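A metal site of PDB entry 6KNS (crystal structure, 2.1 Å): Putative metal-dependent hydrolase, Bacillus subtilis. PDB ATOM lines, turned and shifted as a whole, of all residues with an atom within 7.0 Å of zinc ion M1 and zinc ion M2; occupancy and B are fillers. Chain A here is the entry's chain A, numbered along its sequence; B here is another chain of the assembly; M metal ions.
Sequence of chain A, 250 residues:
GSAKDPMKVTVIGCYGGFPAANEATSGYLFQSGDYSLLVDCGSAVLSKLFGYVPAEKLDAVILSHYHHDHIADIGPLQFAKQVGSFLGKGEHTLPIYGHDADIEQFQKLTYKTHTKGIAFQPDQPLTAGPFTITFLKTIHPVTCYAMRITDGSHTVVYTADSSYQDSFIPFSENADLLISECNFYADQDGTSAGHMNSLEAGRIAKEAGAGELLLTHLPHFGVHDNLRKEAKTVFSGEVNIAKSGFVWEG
ND1 of His 217 lies within hydrogen-bond range of ND2 of Asn 183 (2.7 Å). The side-chain carboxylate of Asp 40 sits at hydrogen-bond distance from a ring nitrogen (ND1) of His 70 (2.7 Å). The side-chain sulfur (SG) of Cys 144 is in hydrogen-bond range of the backbone carbonyl oxygen (O) of Asp 161 (3.7 Å). ND1 of His 65 sits at hydrogen-bond distance from SG of Cys 144 (3.3 Å). A ring nitrogen (ND1) of His 65 lies within hydrogen-bond range of the side-chain hydroxyl of Ser 64 (2.9 Å). A ring nitrogen (ND1) of His 140 is in hydrogen-bond range of the backbone carbonyl oxygen of Gly 194 (2.8 Å). OD2 of Asp 69 lies close to N of Gly 17, at 3.1 Å. The backbone NH of Ser 26 sits at hydrogen-bond distance from the backbone carbonyl oxygen of Asp 69 (3.4 Å).
Of the 27 residues printed, 4 come within 4 Å of zinc ion M1. The nearest printed residue that does not touch zinc ion M1 is His 70 (4.3 Å).
Five residues have an atom within 4 Å of zinc ion M2: His 65, Asp 69, His 70, Asp 161 and His 217. The nearest printed residue that does not touch zinc ion M2 is His 195 (4.6 Å).
Zinc ion M1 is bound by ND1 of His 67 (2.1 Å), NE2 of His 65 (2.3 Å), NE2 of His 140 (2.3 Å) and OD2 of Asp 161 (2.4 Å). Zinc ion M1 has four donor atoms within binding distance.
Zinc ion M2 is bound by a ring nitrogen (NE2) of His 217 (2.1 Å), a ring nitrogen (NE2) of His 70 (2.2 Å), the side-chain carboxylate (OD2) of Asp 161 (2.3 Å) and the side-chain carboxylate (OD2) of Asp 69 (2.5 Å).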
ATOM      1  N   TYR A  15      28.446  10.843  10.774  1.00  0.00           N
ATOM      2  CA  TYR A  15      27.048  10.913  11.217  1.00  0.00           C
ATOM      3  C   TYR A  15      26.097  11.597  10.253  1.00  0.00           C
ATOM      4  O   TYR A  15      26.448  12.584   9.595  1.00  0.00           O
ATOM      5  CB  TYR A  15      26.923  11.552  12.618  1.00  0.00           C
ATOM      6  CG  TYR A  15      27.212  10.538  13.710  1.00  0.00           C
ATOM      7  CD1 TYR A  15      26.193   9.776  14.269  1.00  0.00           C
ATOM      8  CD2 TYR A  15      28.502  10.308  14.133  1.00  0.00           C
ATOM      9  CE1 TYR A  15      26.467   8.813  15.211  1.00  0.00           C
ATOM     10  CE2 TYR A  15      28.798   9.355  15.081  1.00  0.00           C
ATOM     11  CZ  TYR A  15      27.772   8.600  15.605  1.00  0.00           C
ATOM     12  OH  TYR A  15      28.067   7.692  16.579  1.00  0.00           O
ATOM     13  N   GLY A  16      24.867  11.090  10.199  1.00  0.00           N
ATOM     14  CA  GLY A  16      23.852  11.701   9.371  1.00  0.00           C
ATOM     15  C   GLY A  16      23.216  12.860  10.130  1.00  0.00           C
ATOM     16  O   GLY A  16      22.974  12.733  11.303  1.00  0.00           O
ATOM     17  N   GLY A  17      22.945  13.972   9.451  1.00  0.00           N
ATOM     18  CA  GLY A  17      22.148  15.077   9.979  1.00  0.00           C
ATOM     19  C   GLY A  17      22.910  16.081  10.846  1.00  0.00           C
ATOM     20  O   GLY A  17      22.935  17.279  10.536  1.00  0.00           O
ATOM     21  N   SER A  26      29.196  14.250   7.537  1.00  0.00           N
ATOM     22  CA  SER A  26      29.913  13.813   6.353  1.00  0.00           C
ATOM     23  C   SER A  26      31.157  14.603   5.945  1.00  0.00           C
ATOM     24  O   SER A  26      31.108  15.793   5.708  1.00  0.00           O
ATOM     25  CB  SER A  26      28.982  13.726   5.167  1.00  0.00           C
ATOM     26  OG  SER A  26      27.939  12.778   5.401  1.00  0.00           O
ATOM     27  N   ASP A  40      32.878  16.215   0.625  1.00  0.00           N
ATOM     28  CA  ASP A  40      31.931  16.758   1.608  1.00  0.00           C
ATOM     29  C   ASP A  40      32.651  17.382   2.776  1.00  0.00           C
ATOM     30  O   ASP A  40      33.794  17.017   3.106  1.00  0.00           O
ATOM     31  CB  ASP A  40      30.823  15.751   2.020  1.00  0.00           C
ATOM     32  CG  ASP A  40      29.809  15.517   0.885  1.00  0.00           C
ATOM     33  OD1 ASP A  40      29.835  16.282  -0.096  1.00  0.00           O
ATOM     34  OD2 ASP A  40      29.008  14.588   0.942  1.00  0.00           O
ATOM     35  N   SER A  64      28.740  16.669  -2.574  1.00  0.00           N
ATOM     36  CA  SER A  64      27.704  15.831  -3.197  1.00  0.00           C
ATOM     37  C   SER A  64      26.375  16.618  -3.301  1.00  0.00           C
ATOM     38  O   SER A  64      25.640  16.447  -4.284  1.00  0.00           O
ATOM     39  CB  SER A  64      27.445  14.585  -2.372  1.00  0.00           C
ATOM     40  OG  SER A  64      27.093  14.944  -1.029  1.00  0.00           O
ATOM     41  N   HIS A  65      26.088  17.426  -2.297  1.00  0.00           N
ATOM     42  CA  HIS A  65      24.863  18.205  -2.242  1.00  0.00           C
ATOM     43  C   HIS A  65      24.940  19.245  -1.132  1.00  0.00           C
ATOM     44  O   HIS A  65      25.916  19.265  -0.368  1.00  0.00           O
ATOM     45  CB  HIS A  65      23.635  17.308  -2.107  1.00  0.00           C
ATOM     46  CG  HIS A  65      23.473  16.610  -0.784  1.00  0.00           C
ATOM     47  ND1 HIS A  65      24.374  15.676  -0.298  1.00  0.00           N
ATOM     48  CD2 HIS A  65      22.428  16.610   0.091  1.00  0.00           C
ATOM     49  CE1 HIS A  65      23.893  15.168   0.831  1.00  0.00           C
ATOM     50  NE2 HIS A  65      22.726  15.717   1.093  1.00  0.00           N
ATOM     51  N   TYR A  66      23.927  20.102  -1.045  1.00  0.00           N
ATOM     52  CA  TYR A  66      24.018  21.261  -0.194  1.00  0.00           C
ATOM     53  C   TYR A  66      23.209  21.220   1.101  1.00  0.00           C
ATOM     54  O   TYR A  66      22.960  22.254   1.715  1.00  0.00           O
ATOM     55  CB  TYR A  66      23.643  22.497  -1.007  1.00  0.00           C
ATOM     56  CG  TYR A  66      24.553  22.741  -2.236  1.00  0.00           C
ATOM     57  CD1 TYR A  66      25.841  23.204  -2.062  1.00  0.00           C
ATOM     58  CD2 TYR A  66      24.115  22.529  -3.514  1.00  0.00           C
ATOM     59  CE1 TYR A  66      26.673  23.453  -3.122  1.00  0.00           C
ATOM     60  CE2 TYR A  66      24.967  22.791  -4.627  1.00  0.00           C
ATOM     61  CZ  TYR A  66      26.243  23.239  -4.410  1.00  0.00           C
ATOM     62  OH  TYR A  66      27.134  23.535  -5.412  1.00  0.00           O
ATOM     63  N   HIS A  67      22.871  20.032   1.564  1.00  0.00           N
ATOM     64  CA  HIS A  67      22.292  19.862   2.911  1.00  0.00           C
ATOM     65  C   HIS A  67      23.367  20.267   3.940  1.00  0.00           C
ATOM     66  O   HIS A  67      24.552  20.006   3.733  1.00  0.00           O
ATOM     67  CB  HIS A  67      21.877  18.394   3.120  1.00  0.00           C
ATOM     68  CG  HIS A  67      20.471  18.075   2.747  1.00  0.00           C
ATOM     69  ND1 HIS A  67      20.024  16.784   2.567  1.00  0.00           N
ATOM     70  CD2 HIS A  67      19.374  18.875   2.613  1.00  0.00           C
ATOM     71  CE1 HIS A  67      18.725  16.802   2.296  1.00  0.00           C
ATOM     72  NE2 HIS A  67      18.310  18.064   2.313  1.00  0.00           N
ATOM     73  N   HIS A  68      22.928  20.875   5.054  1.00  0.00           N
ATOM     74  CA  HIS A  68      23.816  21.407   6.106  1.00  0.00           C
ATOM     75  C   HIS A  68      24.866  20.435   6.589  1.00  0.00           C
ATOM     76  O   HIS A  68      26.043  20.780   6.784  1.00  0.00           O
ATOM     77  CB  HIS A  68      23.008  21.820   7.331  1.00  0.00           C
ATOM     78  CG  HIS A  68      22.035  22.893   7.081  1.00  0.00           C
ATOM     79  ND1 HIS A  68      22.393  24.127   6.546  1.00  0.00           N
ATOM     80  CD2 HIS A  68      20.685  22.932   7.277  1.00  0.00           C
ATOM     81  CE1 HIS A  68      21.304  24.873   6.452  1.00  0.00           C
ATOM     82  NE2 HIS A  68      20.260  24.171   6.879  1.00  0.00           N
ATOM     83  N   ASP A  69      24.462  19.193   6.788  1.00  0.00           N
ATOM     84  CA  ASP A  69      25.410  18.172   7.252  1.00  0.00           C
ATOM     85  C   ASP A  69      26.497  17.761   6.252  1.00  0.00           C
ATOM     86  O   ASP A  69      27.398  16.984   6.611  1.00  0.00           O
ATOM     87  CB  ASP A  69      24.662  16.965   7.829  1.00  0.00           C
ATOM     88  CG  ASP A  69      23.792  16.268   6.789  1.00  0.00           C
ATOM     89  OD1 ASP A  69      23.087  16.974   6.083  1.00  0.00           O
ATOM     90  OD2 ASP A  69      23.827  15.030   6.720  1.00  0.00           O
ATOM     91  N   HIS A  70      26.469  18.318   5.047  1.00  0.00           N
ATOM     92  CA  HIS A  70      27.538  18.118   4.063  1.00  0.00           C
ATOM     93  C   HIS A  70      28.328  19.385   3.698  1.00  0.00           C
ATOM     94  O   HIS A  70      29.331  19.291   2.982  1.00  0.00           O
ATOM     95  CB  HIS A  70      26.928  17.500   2.788  1.00  0.00           C
ATOM     96  CG  HIS A  70      26.331  16.152   3.057  1.00  0.00           C
ATOM     97  ND1 HIS A  70      26.919  14.978   2.631  1.00  0.00           N
ATOM     98  CD2 HIS A  70      25.252  15.805   3.791  1.00  0.00           C
ATOM     99  CE1 HIS A  70      26.187  13.969   3.086  1.00  0.00           C
ATOM    100  NE2 HIS A  70      25.164  14.449   3.770  1.00  0.00           N
ATOM    101  N   HIS A 140      16.812  11.892  -3.622  1.00  0.00           N
ATOM    102  CA  HIS A 140      16.994  12.611  -2.366  1.00  0.00           C
ATOM    103  C   HIS A 140      16.143  13.892  -2.371  1.00  0.00           C
ATOM    104  O   HIS A 140      15.789  14.376  -3.440  1.00  0.00           O
ATOM    105  CB  HIS A 140      18.486  12.923  -2.203  1.00  0.00           C
ATOM    106  CG  HIS A 140      18.895  13.175  -0.799  1.00  0.00           C
ATOM    107  ND1 HIS A 140      18.625  12.281   0.213  1.00  0.00           N
ATOM    108  CD2 HIS A 140      19.538  14.211  -0.217  1.00  0.00           C
ATOM    109  CE1 HIS A 140      19.089  12.751   1.350  1.00  0.00           C
ATOM    110  NE2 HIS A 140      19.647  13.920   1.113  1.00  0.00           N
ATOM    111  N   PRO A 141      15.752  14.425  -1.205  1.00  0.00           N
ATOM    112  CA  PRO A 141      14.869  15.593  -1.286  1.00  0.00           C
ATOM    113  C   PRO A 141      15.498  16.851  -1.857  1.00  0.00           C
ATOM    114  O   PRO A 141      14.775  17.783  -2.082  1.00  0.00           O
ATOM    115  CB  PRO A 141      14.446  15.837   0.176  1.00  0.00           C
ATOM    116  CG  PRO A 141      14.935  14.690   0.971  1.00  0.00           C
ATOM    117  CD  PRO A 141      15.904  13.916   0.162  1.00  0.00           C
ATOM    118  N   VAL A 142      16.832  16.948  -1.979  1.00  0.00           N
ATOM    119  CA  VAL A 142      17.480  17.987  -2.783  1.00  0.00           C
ATOM    120  C   VAL A 142      18.374  17.294  -3.792  1.00  0.00           C
ATOM    121  O   VAL A 142      18.704  16.121  -3.639  1.00  0.00           O
ATOM    122  CB  VAL A 142      18.322  18.993  -1.952  1.00  0.00           C
ATOM    123  CG1 VAL A 142      17.420  19.837  -1.007  1.00  0.00           C
ATOM    124  CG2 VAL A 142      19.480  18.314  -1.181  1.00  0.00           C
ATOM    125  N   CYS A 144      21.296  15.777  -5.531  1.00  0.00           N
ATOM    126  CA  CYS A 144      22.457  15.195  -4.899  1.00  0.00           C
ATOM    127  C   CYS A 144      23.123  14.254  -5.872  1.00  0.00           C
ATOM    128  O   CYS A 144      22.413  13.618  -6.673  1.00  0.00           O
ATOM    129  CB  CYS A 144      22.054  14.506  -3.569  1.00  0.00           C
ATOM    130  SG  CYS A 144      23.415  13.701  -2.751  1.00  0.00           S
ATOM    131  N   TYR A 158      31.143   6.378  -3.626  1.00  0.00           N
ATOM    132  CA  TYR A 158      30.474   7.056  -2.520  1.00  0.00           C
ATOM    133  C   TYR A 158      29.043   7.329  -2.974  1.00  0.00           C
ATOM    134  O   TYR A 158      28.836   8.006  -3.963  1.00  0.00           O
ATOM    135  CB  TYR A 158      31.170   8.392  -2.258  1.00  0.00           C
ATOM    136  CG  TYR A 158      30.545   9.296  -1.258  1.00  0.00           C
ATOM    137  CD1 TYR A 158      30.145   8.819  -0.010  1.00  0.00           C
ATOM    138  CD2 TYR A 158      30.389  10.672  -1.523  1.00  0.00           C
ATOM    139  CE1 TYR A 158      29.581   9.699   0.963  1.00  0.00           C
ATOM    140  CE2 TYR A 158      29.844  11.547  -0.571  1.00  0.00           C
ATOM    141  CZ  TYR A 158      29.453  11.060   0.660  1.00  0.00           C
ATOM    142  OH  TYR A 158      28.921  11.902   1.603  1.00  0.00           O
ATOM    143  N   ALA A 160      26.885   9.179  -1.580  1.00  0.00           N
ATOM    144  CA  ALA A 160      26.306  10.353  -0.985  1.00  0.00           C
ATOM    145  C   ALA A 160      24.991   9.904  -0.316  1.00  0.00           C
ATOM    146  O   ALA A 160      24.911   8.788   0.230  1.00  0.00           O
ATOM    147  CB  ALA A 160      26.087  11.460  -2.020  1.00  0.00           C
ATOM    148  N   ASP A 161      23.966  10.756  -0.353  1.00  0.00           N
ATOM    149  CA  ASP A 161      22.686  10.439   0.246  1.00  0.00           C
ATOM    150  C   ASP A 161      21.714  10.000  -0.808  1.00  0.00           C
ATOM    151  O   ASP A 161      21.556  10.686  -1.815  1.00  0.00           O
ATOM    152  CB  ASP A 161      22.082  11.669   0.882  1.00  0.00           C
ATOM    153  CG  ASP A 161      22.810  12.110   2.133  1.00  0.00           C
ATOM    154  OD1 ASP A 161      23.958  11.670   2.439  1.00  0.00           O
ATOM    155  OD2 ASP A 161      22.172  12.887   2.819  1.00  0.00           O
ATOM    156  N   SER A 162      21.000   8.919  -0.548  1.00  0.00           N
ATOM    157  CA  SER A 162      19.975   8.455  -1.498  1.00  0.00           C
ATOM    158  C   SER A 162      19.071   7.413  -0.860  1.00  0.00           C
ATOM    159  O   SER A 162      19.496   6.675   0.029  1.00  0.00           O
ATOM    160  CB  SER A 162      20.660   7.814  -2.696  1.00  0.00           C
ATOM    161  OG  SER A 162      19.751   7.548  -3.759  1.00  0.00           O
ATOM    162  N   GLU A 181      25.731   5.286   2.320  1.00  0.00           N
ATOM    163  CA  GLU A 181      24.927   5.815   3.374  1.00  0.00           C
ATOM    164  C   GLU A 181      24.102   4.637   3.916  1.00  0.00           C
ATOM    165  O   GLU A 181      23.804   3.666   3.207  1.00  0.00           O
ATOM    166  CB  GLU A 181      24.071   6.979   2.849  1.00  0.00           C
ATOM    167  CG  GLU A 181      22.813   6.642   2.073  1.00  0.00           C
ATOM    168  CD  GLU A 181      21.579   7.223   2.775  1.00  0.00           C
ATOM    169  OE1 GLU A 181      21.032   6.563   3.694  1.00  0.00           O
ATOM    170  OE2 GLU A 181      21.194   8.368   2.418  1.00  0.00           O
ATOM    171  N   ASN A 183      21.418   5.228   6.823  1.00  0.00           N
ATOM    172  CA  ASN A 183      20.836   5.997   7.904  1.00  0.00           C
ATOM    173  C   ASN A 183      19.732   5.220   8.653  1.00  0.00           C
ATOM    174  O   ASN A 183      19.327   5.668   9.704  1.00  0.00           O
ATOM    175  CB  ASN A 183      20.254   7.304   7.351  1.00  0.00           C
ATOM    176  CG  ASN A 183      20.388   8.474   8.353  1.00  0.00           C
ATOM    177  OD1 ASN A 183      20.188   8.317   9.559  1.00  0.00           O
ATOM    178  ND2 ASN A 183      20.736   9.615   7.853  1.00  0.00           N
ATOM    179  N   ALA A 193      12.468   9.727   3.586  1.00  0.00           N
ATOM    180  CA  ALA A 193      13.568  10.647   3.937  1.00  0.00           C
ATOM    181  C   ALA A 193      14.677  10.722   2.897  1.00  0.00           C
ATOM    182  O   ALA A 193      15.653  11.458   3.091  1.00  0.00           O
ATOM    183  CB  ALA A 193      14.164  10.266   5.325  1.00  0.00           C
ATOM    184  N   GLY A 194      14.596   9.953   1.828  1.00  0.00           N
ATOM    185  CA  GLY A 194      15.688   9.920   0.849  1.00  0.00           C
ATOM    186  C   GLY A 194      16.962   9.238   1.339  1.00  0.00           C
ATOM    187  O   GLY A 194      18.090   9.659   1.001  1.00  0.00           O
ATOM    188  N   HIS A 195      16.775   8.195   2.126  1.00  0.00           N
ATOM    189  CA  HIS A 195      17.888   7.413   2.682  1.00  0.00           C
ATOM    190  C   HIS A 195      17.716   5.910   2.471  1.00  0.00           C
ATOM    191  O   HIS A 195      16.670   5.423   2.065  1.00  0.00           O
ATOM    192  CB  HIS A 195      18.061   7.686   4.181  1.00  0.00           C
ATOM    193  CG  HIS A 195      18.484   9.082   4.495  1.00  0.00           C
ATOM    194  ND1 HIS A 195      19.623   9.664   3.971  1.00  0.00           N
ATOM    195  CD2 HIS A 195      17.924  10.015   5.303  1.00  0.00           C
ATOM    196  CE1 HIS A 195      19.747  10.888   4.452  1.00  0.00           C
ATOM    197  NE2 HIS A 195      18.712  11.143   5.231  1.00  0.00           N
ATOM    198  N   HIS A 217      26.902   7.692   7.319  1.00  0.00           N
ATOM    199  CA  HIS A 217      25.731   8.562   7.474  1.00  0.00           C
ATOM    200  C   HIS A 217      24.817   7.975   8.521  1.00  0.00           C
ATOM    201  O   HIS A 217      23.618   7.824   8.315  1.00  0.00           O
ATOM    202  CB  HIS A 217      25.014   8.738   6.149  1.00  0.00           C
ATOM    203  CG  HIS A 217      24.316  10.039   6.014  1.00  0.00           C
ATOM    204  ND1 HIS A 217      23.028  10.239   6.480  1.00  0.00           N
ATOM    205  CD2 HIS A 217      24.736  11.215   5.501  1.00  0.00           C
ATOM    206  CE1 HIS A 217      22.672  11.487   6.208  1.00  0.00           C
ATOM    207  NE2 HIS A 217      23.697  12.104   5.623  1.00  0.00           N
ATOM    208  N   PHE B  79      18.912  20.623  11.956  1.00  0.00           N
ATOM    209  CA  PHE B  79      18.676  19.218  11.713  1.00  0.00           C
ATOM    210  C   PHE B  79      18.621  18.392  13.019  1.00  0.00           C
ATOM    211  O   PHE B  79      17.829  17.466  13.102  1.00  0.00           O
ATOM    212  CB  PHE B  79      19.704  18.656  10.757  1.00  0.00           C
ATOM    213  CG  PHE B  79      19.516  19.075   9.306  1.00  0.00           C
ATOM    214  CD1 PHE B  79      18.372  19.777   8.867  1.00  0.00           C
ATOM    215  CD2 PHE B  79      20.459  18.677   8.348  1.00  0.00           C
ATOM    216  CE1 PHE B  79      18.214  20.124   7.518  1.00  0.00           C
ATOM    217  CE2 PHE B  79      20.288  19.018   6.989  1.00  0.00           C
ATOM    218  CZ  PHE B  79      19.161  19.735   6.580  1.00  0.00           C
HETATM  219 ZN    ZN M   1      21.108  14.977   2.483  1.00  0.00          ZN
HETATM  220 ZN    ZN M   2      23.215  13.865   4.561  1.00  0.00          ZN
